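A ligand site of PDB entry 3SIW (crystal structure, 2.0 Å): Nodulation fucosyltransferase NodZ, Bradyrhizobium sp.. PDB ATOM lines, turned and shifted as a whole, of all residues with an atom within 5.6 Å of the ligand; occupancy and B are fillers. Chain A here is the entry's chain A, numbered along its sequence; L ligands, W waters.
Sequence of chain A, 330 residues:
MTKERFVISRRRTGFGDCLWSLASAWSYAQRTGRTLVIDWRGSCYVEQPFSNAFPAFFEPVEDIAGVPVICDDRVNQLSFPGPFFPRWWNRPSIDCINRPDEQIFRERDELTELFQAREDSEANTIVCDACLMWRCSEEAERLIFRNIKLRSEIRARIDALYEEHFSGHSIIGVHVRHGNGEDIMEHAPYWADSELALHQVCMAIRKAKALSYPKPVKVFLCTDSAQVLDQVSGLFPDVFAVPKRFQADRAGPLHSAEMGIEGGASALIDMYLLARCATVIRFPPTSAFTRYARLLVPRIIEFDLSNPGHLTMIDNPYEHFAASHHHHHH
The side-chain hydroxyl (OG) of Ser 287 is in hydrogen-bond range of the backbone NH (N) of Phe 289 (3.1 Å).
The backbone carbonyl oxygen of Gly 14 lies within hydrogen-bond range of the side-chain sulfur of Cys 18 (3.4 Å).
N of Val 176 sits at hydrogen-bond distance from O of Cys 222, at 3.0 Å.
The backbone NH (N) of Gly 16 lies within hydrogen-bond range of the side-chain sulfur (SD) of Met 271, 3.7 Å away.
The side-chain carboxylate of Asp 270 lies close to the side-chain sulfur of Cys 222 (3.7 Å).
OH of Tyr 45 is in hydrogen-bond range of N of Phe 15 (3.2 Å).
OG1 of Thr 13 is in hydrogen-bond range of OD2 of Asp 17.
The guanidinium group (NE) of Arg 177 lies within salt-bridge range of the side-chain carboxylate (OD2) of Asp 224, at 2.9 Å.
Water W1 lies within hydrogen-bond range of the backbone carbonyl oxygen of Gly 263 (2.8 Å), a nitrogen (N4) of the ligand (2.9 Å) and the backbone NH of Ala 267 (3.5 Å).
An oxygen (O11) of the ligand lies close to the backbone carbonyl oxygen (O) of Cys 222 (3.2 Å).
Residues that only touch the ligand: Gly 14 (3.4 Å), Asp 224 (3.7 Å), Ser 266 (3.5 Å) and Ala 267 (3.4 Å).
Hydrophobic or aromatic side chains that line the ligand: Tyr 45, His 175, Ala 267, Ala 288 and Phe 289.
16 residues have an atom within 4 Å of the ligand: Gly 14, Phe 15, Gly 16, Asp 17, Tyr 45, His 175, Arg 177, Cys 222, Thr 223, Asp 224, Ser 266, Ala 267, Asp 270, Ser 287, Ala 288 and Phe 289.
The nearest printed residue that does not touch the ligand is Thr 286 (4.1 Å).
The side-chain carboxylate of Asp 270 is in hydrogen-bond range of a nitrogen (N3) of the ligand (2.8 Å).
N of Thr 223 lies within hydrogen-bond range of O11 of the ligand.
O1 of the ligand sits at hydrogen-bond distance from N of Ala 288 (2.9 Å).
The guanidinium group (NH1) of Arg 177 is in salt-bridge range of an oxygen (O3) of the ligand (2.9 Å).
OG of Ser 287 sits at hydrogen-bond distance from O2 of the ligand (2.6 Å).
O9 of the ligand is in hydrogen-bond range of N of Phe 15 (3.3 Å).
O6 of the ligand is in hydrogen-bond range of N of Asp 17 (3.1 Å).
N of Gly 16 lies within hydrogen-bond range of O5 of the ligand, at 3.1 Å.
The side-chain hydroxyl (OH) of Tyr 45 lies within hydrogen-bond range of an oxygen (O10) of the ligand, at 2.6 Å.
NE2 of His 175 is in hydrogen-bond range of N2 of the ligand, at 2.8 Å.
The backbone NH (N) of Phe 289 lies within hydrogen-bond range of an oxygen (O4) of the ligand (3.3 Å).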
ATOM      1  N   THR A  13      -6.668   7.182   5.141  1.00  0.00           N
ATOM      2  CA  THR A  13      -6.487   8.454   5.844  1.00  0.00           C
ATOM      3  C   THR A  13      -6.490   9.606   4.820  1.00  0.00           C
ATOM      4  O   THR A  13      -7.079   9.511   3.720  1.00  0.00           O
ATOM      5  CB  THR A  13      -5.159   8.390   6.659  1.00  0.00           C
ATOM      6  OG1 THR A  13      -4.061   8.064   5.790  1.00  0.00           O
ATOM      7  CG2 THR A  13      -5.254   7.313   7.690  1.00  0.00           C
ATOM      8  N   GLY A  14      -5.820  10.700   5.125  1.00  0.00           N
ATOM      9  CA  GLY A  14      -5.780  11.798   4.211  1.00  0.00           C
ATOM     10  C   GLY A  14      -5.003  11.461   2.968  1.00  0.00           C
ATOM     11  O   GLY A  14      -4.124  10.578   2.994  1.00  0.00           O
ATOM     12  N   PHE A  15      -5.283  12.179   1.887  1.00  0.00           N
ATOM     13  CA  PHE A  15      -4.671  11.841   0.650  1.00  0.00           C
ATOM     14  C   PHE A  15      -3.135  11.908   0.618  1.00  0.00           C
ATOM     15  O   PHE A  15      -2.493  11.165  -0.115  1.00  0.00           O
ATOM     16  CB  PHE A  15      -5.218  12.709  -0.466  1.00  0.00           C
ATOM     17  CG  PHE A  15      -6.608  12.375  -0.861  1.00  0.00           C
ATOM     18  CD1 PHE A  15      -6.902  11.140  -1.361  1.00  0.00           C
ATOM     19  CD2 PHE A  15      -7.600  13.295  -0.749  1.00  0.00           C
ATOM     20  CE1 PHE A  15      -8.209  10.810  -1.712  1.00  0.00           C
ATOM     21  CE2 PHE A  15      -8.899  12.982  -1.112  1.00  0.00           C
ATOM     22  CZ  PHE A  15      -9.182  11.741  -1.606  1.00  0.00           C
ATOM     23  N   GLY A  16      -2.551  12.828   1.373  1.00  0.00           N
ATOM     24  CA  GLY A  16      -1.079  13.002   1.379  1.00  0.00           C
ATOM     25  C   GLY A  16      -0.457  11.674   1.810  1.00  0.00           C
ATOM     26  O   GLY A  16       0.483  11.147   1.191  1.00  0.00           O
ATOM     27  N   ASP A  17      -0.983  11.154   2.904  1.00  0.00           N
ATOM     28  CA  ASP A  17      -0.570   9.856   3.432  1.00  0.00           C
ATOM     29  C   ASP A  17      -0.859   8.741   2.435  1.00  0.00           C
ATOM     30  O   ASP A  17       0.029   7.969   2.123  1.00  0.00           O
ATOM     31  CB  ASP A  17      -1.286   9.662   4.801  1.00  0.00           C
ATOM     32  CG  ASP A  17      -0.840   8.432   5.555  1.00  0.00           C
ATOM     33  OD1 ASP A  17      -0.143   7.543   4.998  1.00  0.00           O
ATOM     34  OD2 ASP A  17      -1.225   8.346   6.755  1.00  0.00           O
ATOM     35  N   CYS A  18      -2.091   8.658   1.930  1.00  0.00           N
ATOM     36  CA  CYS A  18      -2.465   7.640   0.968  1.00  0.00           C
ATOM     37  C   CYS A  18      -1.524   7.589  -0.238  1.00  0.00           C
ATOM     38  O   CYS A  18      -1.071   6.510  -0.587  1.00  0.00           O
ATOM     39  CB  CYS A  18      -3.895   7.824   0.461  1.00  0.00           C
ATOM     40  SG  CYS A  18      -5.107   7.588   1.784  1.00  0.00           S
ATOM     41  N   TYR A  45     -13.142   9.537   3.202  1.00  0.00           N
ATOM     42  CA  TYR A  45     -13.972  10.386   2.315  1.00  0.00           C
ATOM     43  C   TYR A  45     -15.174   9.723   1.615  1.00  0.00           C
ATOM     44  O   TYR A  45     -15.902  10.393   0.886  1.00  0.00           O
ATOM     45  CB  TYR A  45     -13.119  10.974   1.213  1.00  0.00           C
ATOM     46  CG  TYR A  45     -11.845  11.664   1.654  1.00  0.00           C
ATOM     47  CD1 TYR A  45     -11.858  12.942   2.246  1.00  0.00           C
ATOM     48  CD2 TYR A  45     -10.653  11.039   1.493  1.00  0.00           C
ATOM     49  CE1 TYR A  45     -10.607  13.576   2.630  1.00  0.00           C
ATOM     50  CE2 TYR A  45      -9.446  11.639   1.859  1.00  0.00           C
ATOM     51  CZ  TYR A  45      -9.425  12.899   2.406  1.00  0.00           C
ATOM     52  OH  TYR A  45      -8.167  13.406   2.707  1.00  0.00           O
ATOM     53  N   MET A 133       4.864   6.402   4.817  1.00  0.00           N
ATOM     54  CA  MET A 133       5.543   7.647   4.550  1.00  0.00           C
ATOM     55  C   MET A 133       7.000   7.432   4.854  1.00  0.00           C
ATOM     56  O   MET A 133       7.332   6.676   5.713  1.00  0.00           O
ATOM     57  CB  MET A 133       4.951   8.790   5.411  1.00  0.00           C
ATOM     58  CG  MET A 133       3.580   9.192   4.860  1.00  0.00           C
ATOM     59  SD  MET A 133       2.654  10.160   6.099  1.00  0.00           S
ATOM     60  CE  MET A 133       3.890  11.333   6.692  1.00  0.00           C
ATOM     61  N   HIS A 175      -0.377  26.510   4.307  1.00  0.00           N
ATOM     62  CA  HIS A 175      -1.121  25.440   4.850  1.00  0.00           C
ATOM     63  C   HIS A 175      -1.103  25.553   6.360  1.00  0.00           C
ATOM     64  O   HIS A 175      -0.052  25.523   7.000  1.00  0.00           O
ATOM     65  CB  HIS A 175      -0.566  24.064   4.408  1.00  0.00           C
ATOM     66  CG  HIS A 175      -1.356  22.914   4.943  1.00  0.00           C
ATOM     67  ND1 HIS A 175      -0.780  21.862   5.614  1.00  0.00           N
ATOM     68  CD2 HIS A 175      -2.689  22.660   4.914  1.00  0.00           C
ATOM     69  CE1 HIS A 175      -1.723  21.001   5.961  1.00  0.00           C
ATOM     70  NE2 HIS A 175      -2.890  21.455   5.542  1.00  0.00           N
ATOM     71  N   VAL A 176      -2.290  25.650   6.922  1.00  0.00           N
ATOM     72  CA  VAL A 176      -2.465  25.665   8.348  1.00  0.00           C
ATOM     73  C   VAL A 176      -3.387  24.554   8.772  1.00  0.00           C
ATOM     74  O   VAL A 176      -4.626  24.594   8.584  1.00  0.00           O
ATOM     75  CB  VAL A 176      -3.040  27.003   8.838  1.00  0.00           C
ATOM     76  CG1 VAL A 176      -3.196  26.970  10.394  1.00  0.00           C
ATOM     77  CG2 VAL A 176      -2.164  28.165   8.337  1.00  0.00           C
ATOM     78  N   ARG A 177      -2.770  23.528   9.334  1.00  0.00           N
ATOM     79  CA  ARG A 177      -3.489  22.346   9.746  1.00  0.00           C
ATOM     80  C   ARG A 177      -3.776  22.510  11.209  1.00  0.00           C
ATOM     81  O   ARG A 177      -2.848  22.707  12.009  1.00  0.00           O
ATOM     82  CB  ARG A 177      -2.599  21.127   9.488  1.00  0.00           C
ATOM     83  CG  ARG A 177      -3.183  19.817   9.919  1.00  0.00           C
ATOM     84  CD  ARG A 177      -3.828  19.066   8.769  1.00  0.00           C
ATOM     85  NE  ARG A 177      -5.071  18.467   9.257  1.00  0.00           N
ATOM     86  CZ  ARG A 177      -5.235  17.231   9.710  1.00  0.00           C
ATOM     87  NH1 ARG A 177      -4.244  16.343   9.706  1.00  0.00           N
ATOM     88  NH2 ARG A 177      -6.431  16.879  10.138  1.00  0.00           N
ATOM     89  N   CYS A 222      -4.823  27.544   2.705  1.00  0.00           N
ATOM     90  CA  CYS A 222      -5.470  26.236   2.808  1.00  0.00           C
ATOM     91  C   CYS A 222      -5.506  25.859   4.274  1.00  0.00           C
ATOM     92  O   CYS A 222      -4.478  25.661   4.894  1.00  0.00           O
ATOM     93  CB  CYS A 222      -4.697  25.175   2.035  1.00  0.00           C
ATOM     94  SG  CYS A 222      -4.608  25.567   0.317  1.00  0.00           S
ATOM     95  N   THR A 223      -6.686  25.785   4.836  1.00  0.00           N
ATOM     96  CA  THR A 223      -6.797  25.489   6.226  1.00  0.00           C
ATOM     97  C   THR A 223      -8.062  24.726   6.395  1.00  0.00           C
ATOM     98  O   THR A 223      -8.987  24.835   5.575  1.00  0.00           O
ATOM     99  CB  THR A 223      -6.853  26.773   7.090  1.00  0.00           C
ATOM    100  OG1 THR A 223      -6.990  26.417   8.454  1.00  0.00           O
ATOM    101  CG2 THR A 223      -8.023  27.710   6.681  1.00  0.00           C
ATOM    102  N   ASP A 224      -8.136  23.980   7.476  1.00  0.00           N
ATOM    103  CA  ASP A 224      -9.341  23.237   7.763  1.00  0.00           C
ATOM    104  C   ASP A 224     -10.151  23.965   8.812  1.00  0.00           C
ATOM    105  O   ASP A 224     -11.166  23.455   9.263  1.00  0.00           O
ATOM    106  CB  ASP A 224      -8.958  21.789   8.158  1.00  0.00           C
ATOM    107  CG  ASP A 224      -7.671  21.721   9.072  1.00  0.00           C
ATOM    108  OD1 ASP A 224      -7.302  22.745   9.718  1.00  0.00           O
ATOM    109  OD2 ASP A 224      -7.054  20.618   9.152  1.00  0.00           O
ATOM    110  N   LYS A 244     -15.043  26.387   0.778  1.00  0.00           N
ATOM    111  CA  LYS A 244     -14.981  25.110   1.520  1.00  0.00           C
ATOM    112  C   LYS A 244     -14.054  23.994   1.040  1.00  0.00           C
ATOM    113  O   LYS A 244     -12.790  24.185   1.006  1.00  0.00           O
ATOM    114  CB  LYS A 244     -16.384  24.598   1.804  1.00  0.00           C
ATOM    115  CG  LYS A 244     -16.895  25.051   3.158  1.00  0.00           C
ATOM    116  CD  LYS A 244     -17.945  24.023   3.728  1.00  0.00           C
ATOM    117  CE  LYS A 244     -17.824  23.898   5.275  1.00  0.00           C
ATOM    118  NZ  LYS A 244     -16.714  22.959   5.663  1.00  0.00           N
ATOM    119  N   GLY A 263     -15.782  16.758   0.330  1.00  0.00           N
ATOM    120  CA  GLY A 263     -14.610  16.971   1.203  1.00  0.00           C
ATOM    121  C   GLY A 263     -13.318  16.468   0.554  1.00  0.00           C
ATOM    122  O   GLY A 263     -12.279  17.124   0.589  1.00  0.00           O
ATOM    123  N   SER A 266     -12.303  18.736  -2.355  1.00  0.00           N
ATOM    124  CA  SER A 266     -11.767  19.999  -1.845  1.00  0.00           C
ATOM    125  C   SER A 266     -10.332  19.823  -1.340  1.00  0.00           C
ATOM    126  O   SER A 266      -9.468  20.671  -1.573  1.00  0.00           O
ATOM    127  CB  SER A 266     -12.683  20.565  -0.744  1.00  0.00           C
ATOM    128  OG  SER A 266     -13.889  21.051  -1.318  1.00  0.00           O
ATOM    129  N   ALA A 267     -10.064  18.700  -0.677  1.00  0.00           N
ATOM    130  CA  ALA A 267      -8.697  18.393  -0.206  1.00  0.00           C
ATOM    131  C   ALA A 267      -7.726  18.316  -1.391  1.00  0.00           C
ATOM    132  O   ALA A 267      -6.643  18.917  -1.374  1.00  0.00           O
ATOM    133  CB  ALA A 267      -8.677  17.085   0.614  1.00  0.00           C
ATOM    134  N   ASP A 270      -6.954  21.688  -3.036  1.00  0.00           N
ATOM    135  CA  ASP A 270      -5.989  22.409  -2.194  1.00  0.00           C
ATOM    136  C   ASP A 270      -4.565  21.850  -2.308  1.00  0.00           C
ATOM    137  O   ASP A 270      -3.631  22.586  -2.519  1.00  0.00           O
ATOM    138  CB  ASP A 270      -6.431  22.443  -0.733  1.00  0.00           C
ATOM    139  CG  ASP A 270      -7.467  23.522  -0.429  1.00  0.00           C
ATOM    140  OD1 ASP A 270      -7.725  24.377  -1.278  1.00  0.00           O
ATOM    141  OD2 ASP A 270      -8.027  23.547   0.712  1.00  0.00           O
ATOM    142  N   MET A 271      -4.409  20.524  -2.283  1.00  0.00           N
ATOM    143  CA  MET A 271      -3.117  19.850  -2.365  1.00  0.00           C
ATOM    144  C   MET A 271      -2.399  20.197  -3.675  1.00  0.00           C
ATOM    145  O   MET A 271      -1.208  20.487  -3.678  1.00  0.00           O
ATOM    146  CB  MET A 271      -3.285  18.312  -2.201  1.00  0.00           C
ATOM    147  CG  MET A 271      -2.286  17.609  -1.241  1.00  0.00           C
ATOM    148  SD  MET A 271      -2.342  15.746  -0.961  1.00  0.00           S
ATOM    149  CE  MET A 271      -2.374  15.257  -2.684  1.00  0.00           C
ATOM    150  N   THR A 286       5.451  18.498   9.099  1.00  0.00           N
ATOM    151  CA  THR A 286       5.246  17.072   9.228  1.00  0.00           C
ATOM    152  C   THR A 286       3.984  16.605   8.484  1.00  0.00           C
ATOM    153  O   THR A 286       3.716  15.412   8.433  1.00  0.00           O
ATOM    154  CB  THR A 286       5.041  16.730  10.693  1.00  0.00           C
ATOM    155  OG1 THR A 286       4.119  17.701  11.250  1.00  0.00           O
ATOM    156  CG2 THR A 286       6.390  16.812  11.464  1.00  0.00           C
ATOM    157  N   SER A 287       3.174  17.533   7.965  1.00  0.00           N
ATOM    158  CA  SER A 287       1.934  17.127   7.364  1.00  0.00           C
ATOM    159  C   SER A 287       2.219  16.581   5.960  1.00  0.00           C
ATOM    160  O   SER A 287       2.928  17.213   5.199  1.00  0.00           O
ATOM    161  CB  SER A 287       0.978  18.308   7.262  1.00  0.00           C
ATOM    162  OG  SER A 287      -0.094  17.989   6.412  1.00  0.00           O
ATOM    163  N   ALA A 288       1.677  15.417   5.648  1.00  0.00           N
ATOM    164  CA  ALA A 288       1.767  14.859   4.293  1.00  0.00           C
ATOM    165  C   ALA A 288       0.973  15.627   3.283  1.00  0.00           C
ATOM    166  O   ALA A 288       1.178  15.456   2.084  1.00  0.00           O
ATOM    167  CB  ALA A 288       1.363  13.354   4.289  1.00  0.00           C
ATOM    168  N   PHE A 289       0.064  16.510   3.736  1.00  0.00           N
ATOM    169  CA  PHE A 289      -0.769  17.229   2.845  1.00  0.00           C
ATOM    170  C   PHE A 289       0.061  18.117   1.933  1.00  0.00           C
ATOM    171  O   PHE A 289      -0.285  18.311   0.768  1.00  0.00           O
ATOM    172  CB  PHE A 289      -1.741  18.107   3.639  1.00  0.00           C
ATOM    173  CG  PHE A 289      -2.790  18.727   2.832  1.00  0.00           C
ATOM    174  CD1 PHE A 289      -2.763  20.043   2.539  1.00  0.00           C
ATOM    175  CD2 PHE A 289      -3.843  17.937   2.349  1.00  0.00           C
ATOM    176  CE1 PHE A 289      -3.770  20.613   1.800  1.00  0.00           C
ATOM    177  CE2 PHE A 289      -4.851  18.497   1.621  1.00  0.00           C
ATOM    178  CZ  PHE A 289      -4.821  19.832   1.370  1.00  0.00           C
HETATM  179  P1  LIG L   1      -1.591  15.210   7.568  1.00  0.00           P
HETATM  180  O1  LIG L   1      -0.167  14.404   7.603  1.00  0.00           O
HETATM  181  O2  LIG L   1      -1.668  16.658   8.020  1.00  0.00           O
HETATM  182  O3  LIG L   1      -2.592  14.294   8.455  1.00  0.00           O
HETATM  183  O4  LIG L   1      -1.982  15.202   5.932  1.00  0.00           O
HETATM  184  P2  LIG L   1      -2.894  14.173   5.089  1.00  0.00           P
HETATM  185  O5  LIG L   1      -3.119  14.767   3.717  1.00  0.00           O
HETATM  186  O6  LIG L   1      -2.406  12.788   5.150  1.00  0.00           O
HETATM  187  O7  LIG L   1      -4.307  14.268   6.030  1.00  0.00           O
HETATM  188  C1  LIG L   1      -4.926  15.525   6.192  1.00  0.00           C
HETATM  189  C2  LIG L   1      -6.347  15.533   5.664  1.00  0.00           C
HETATM  190  O8  LIG L   1      -7.086  16.590   6.403  1.00  0.00           O
HETATM  191  C3  LIG L   1      -6.155  16.089   4.277  1.00  0.00           C
HETATM  192  O9  LIG L   1      -5.925  15.122   3.258  1.00  0.00           O
HETATM  193  C4  LIG L   1      -7.515  16.739   4.063  1.00  0.00           C
HETATM  194  O10 LIG L   1      -8.536  15.711   3.824  1.00  0.00           O
HETATM  195  C5  LIG L   1      -7.717  17.464   5.424  1.00  0.00           C
HETATM  196  N1  LIG L   1      -6.974  18.728   5.348  1.00  0.00           N
HETATM  197  C6  LIG L   1      -5.850  19.100   6.011  1.00  0.00           C
HETATM  198  N2  LIG L   1      -5.496  20.335   5.617  1.00  0.00           N
HETATM  199  C7  LIG L   1      -6.343  20.740   4.664  1.00  0.00           C
HETATM  200  C8  LIG L   1      -6.479  21.892   3.890  1.00  0.00           C
HETATM  201  O11 LIG L   1      -5.704  22.841   3.970  1.00  0.00           O
HETATM  202  N3  LIG L   1      -7.528  21.970   2.943  1.00  0.00           N
HETATM  203  C9  LIG L   1      -8.429  20.914   2.830  1.00  0.00           C
HETATM  204  N4  LIG L   1      -9.451  20.976   1.946  1.00  0.00           N
HETATM  205  N5  LIG L   1      -8.284  19.843   3.614  1.00  0.00           N
HETATM  206  C10 LIG L   1      -7.281  19.720   4.491  1.00  0.00           C
HETATM  207  O   HOH W   1     -11.555  19.091   2.445  1.00  0.00           O
HETATM  208  O   HOH W   2     -10.724  17.135   4.008  1.00  0.00           O
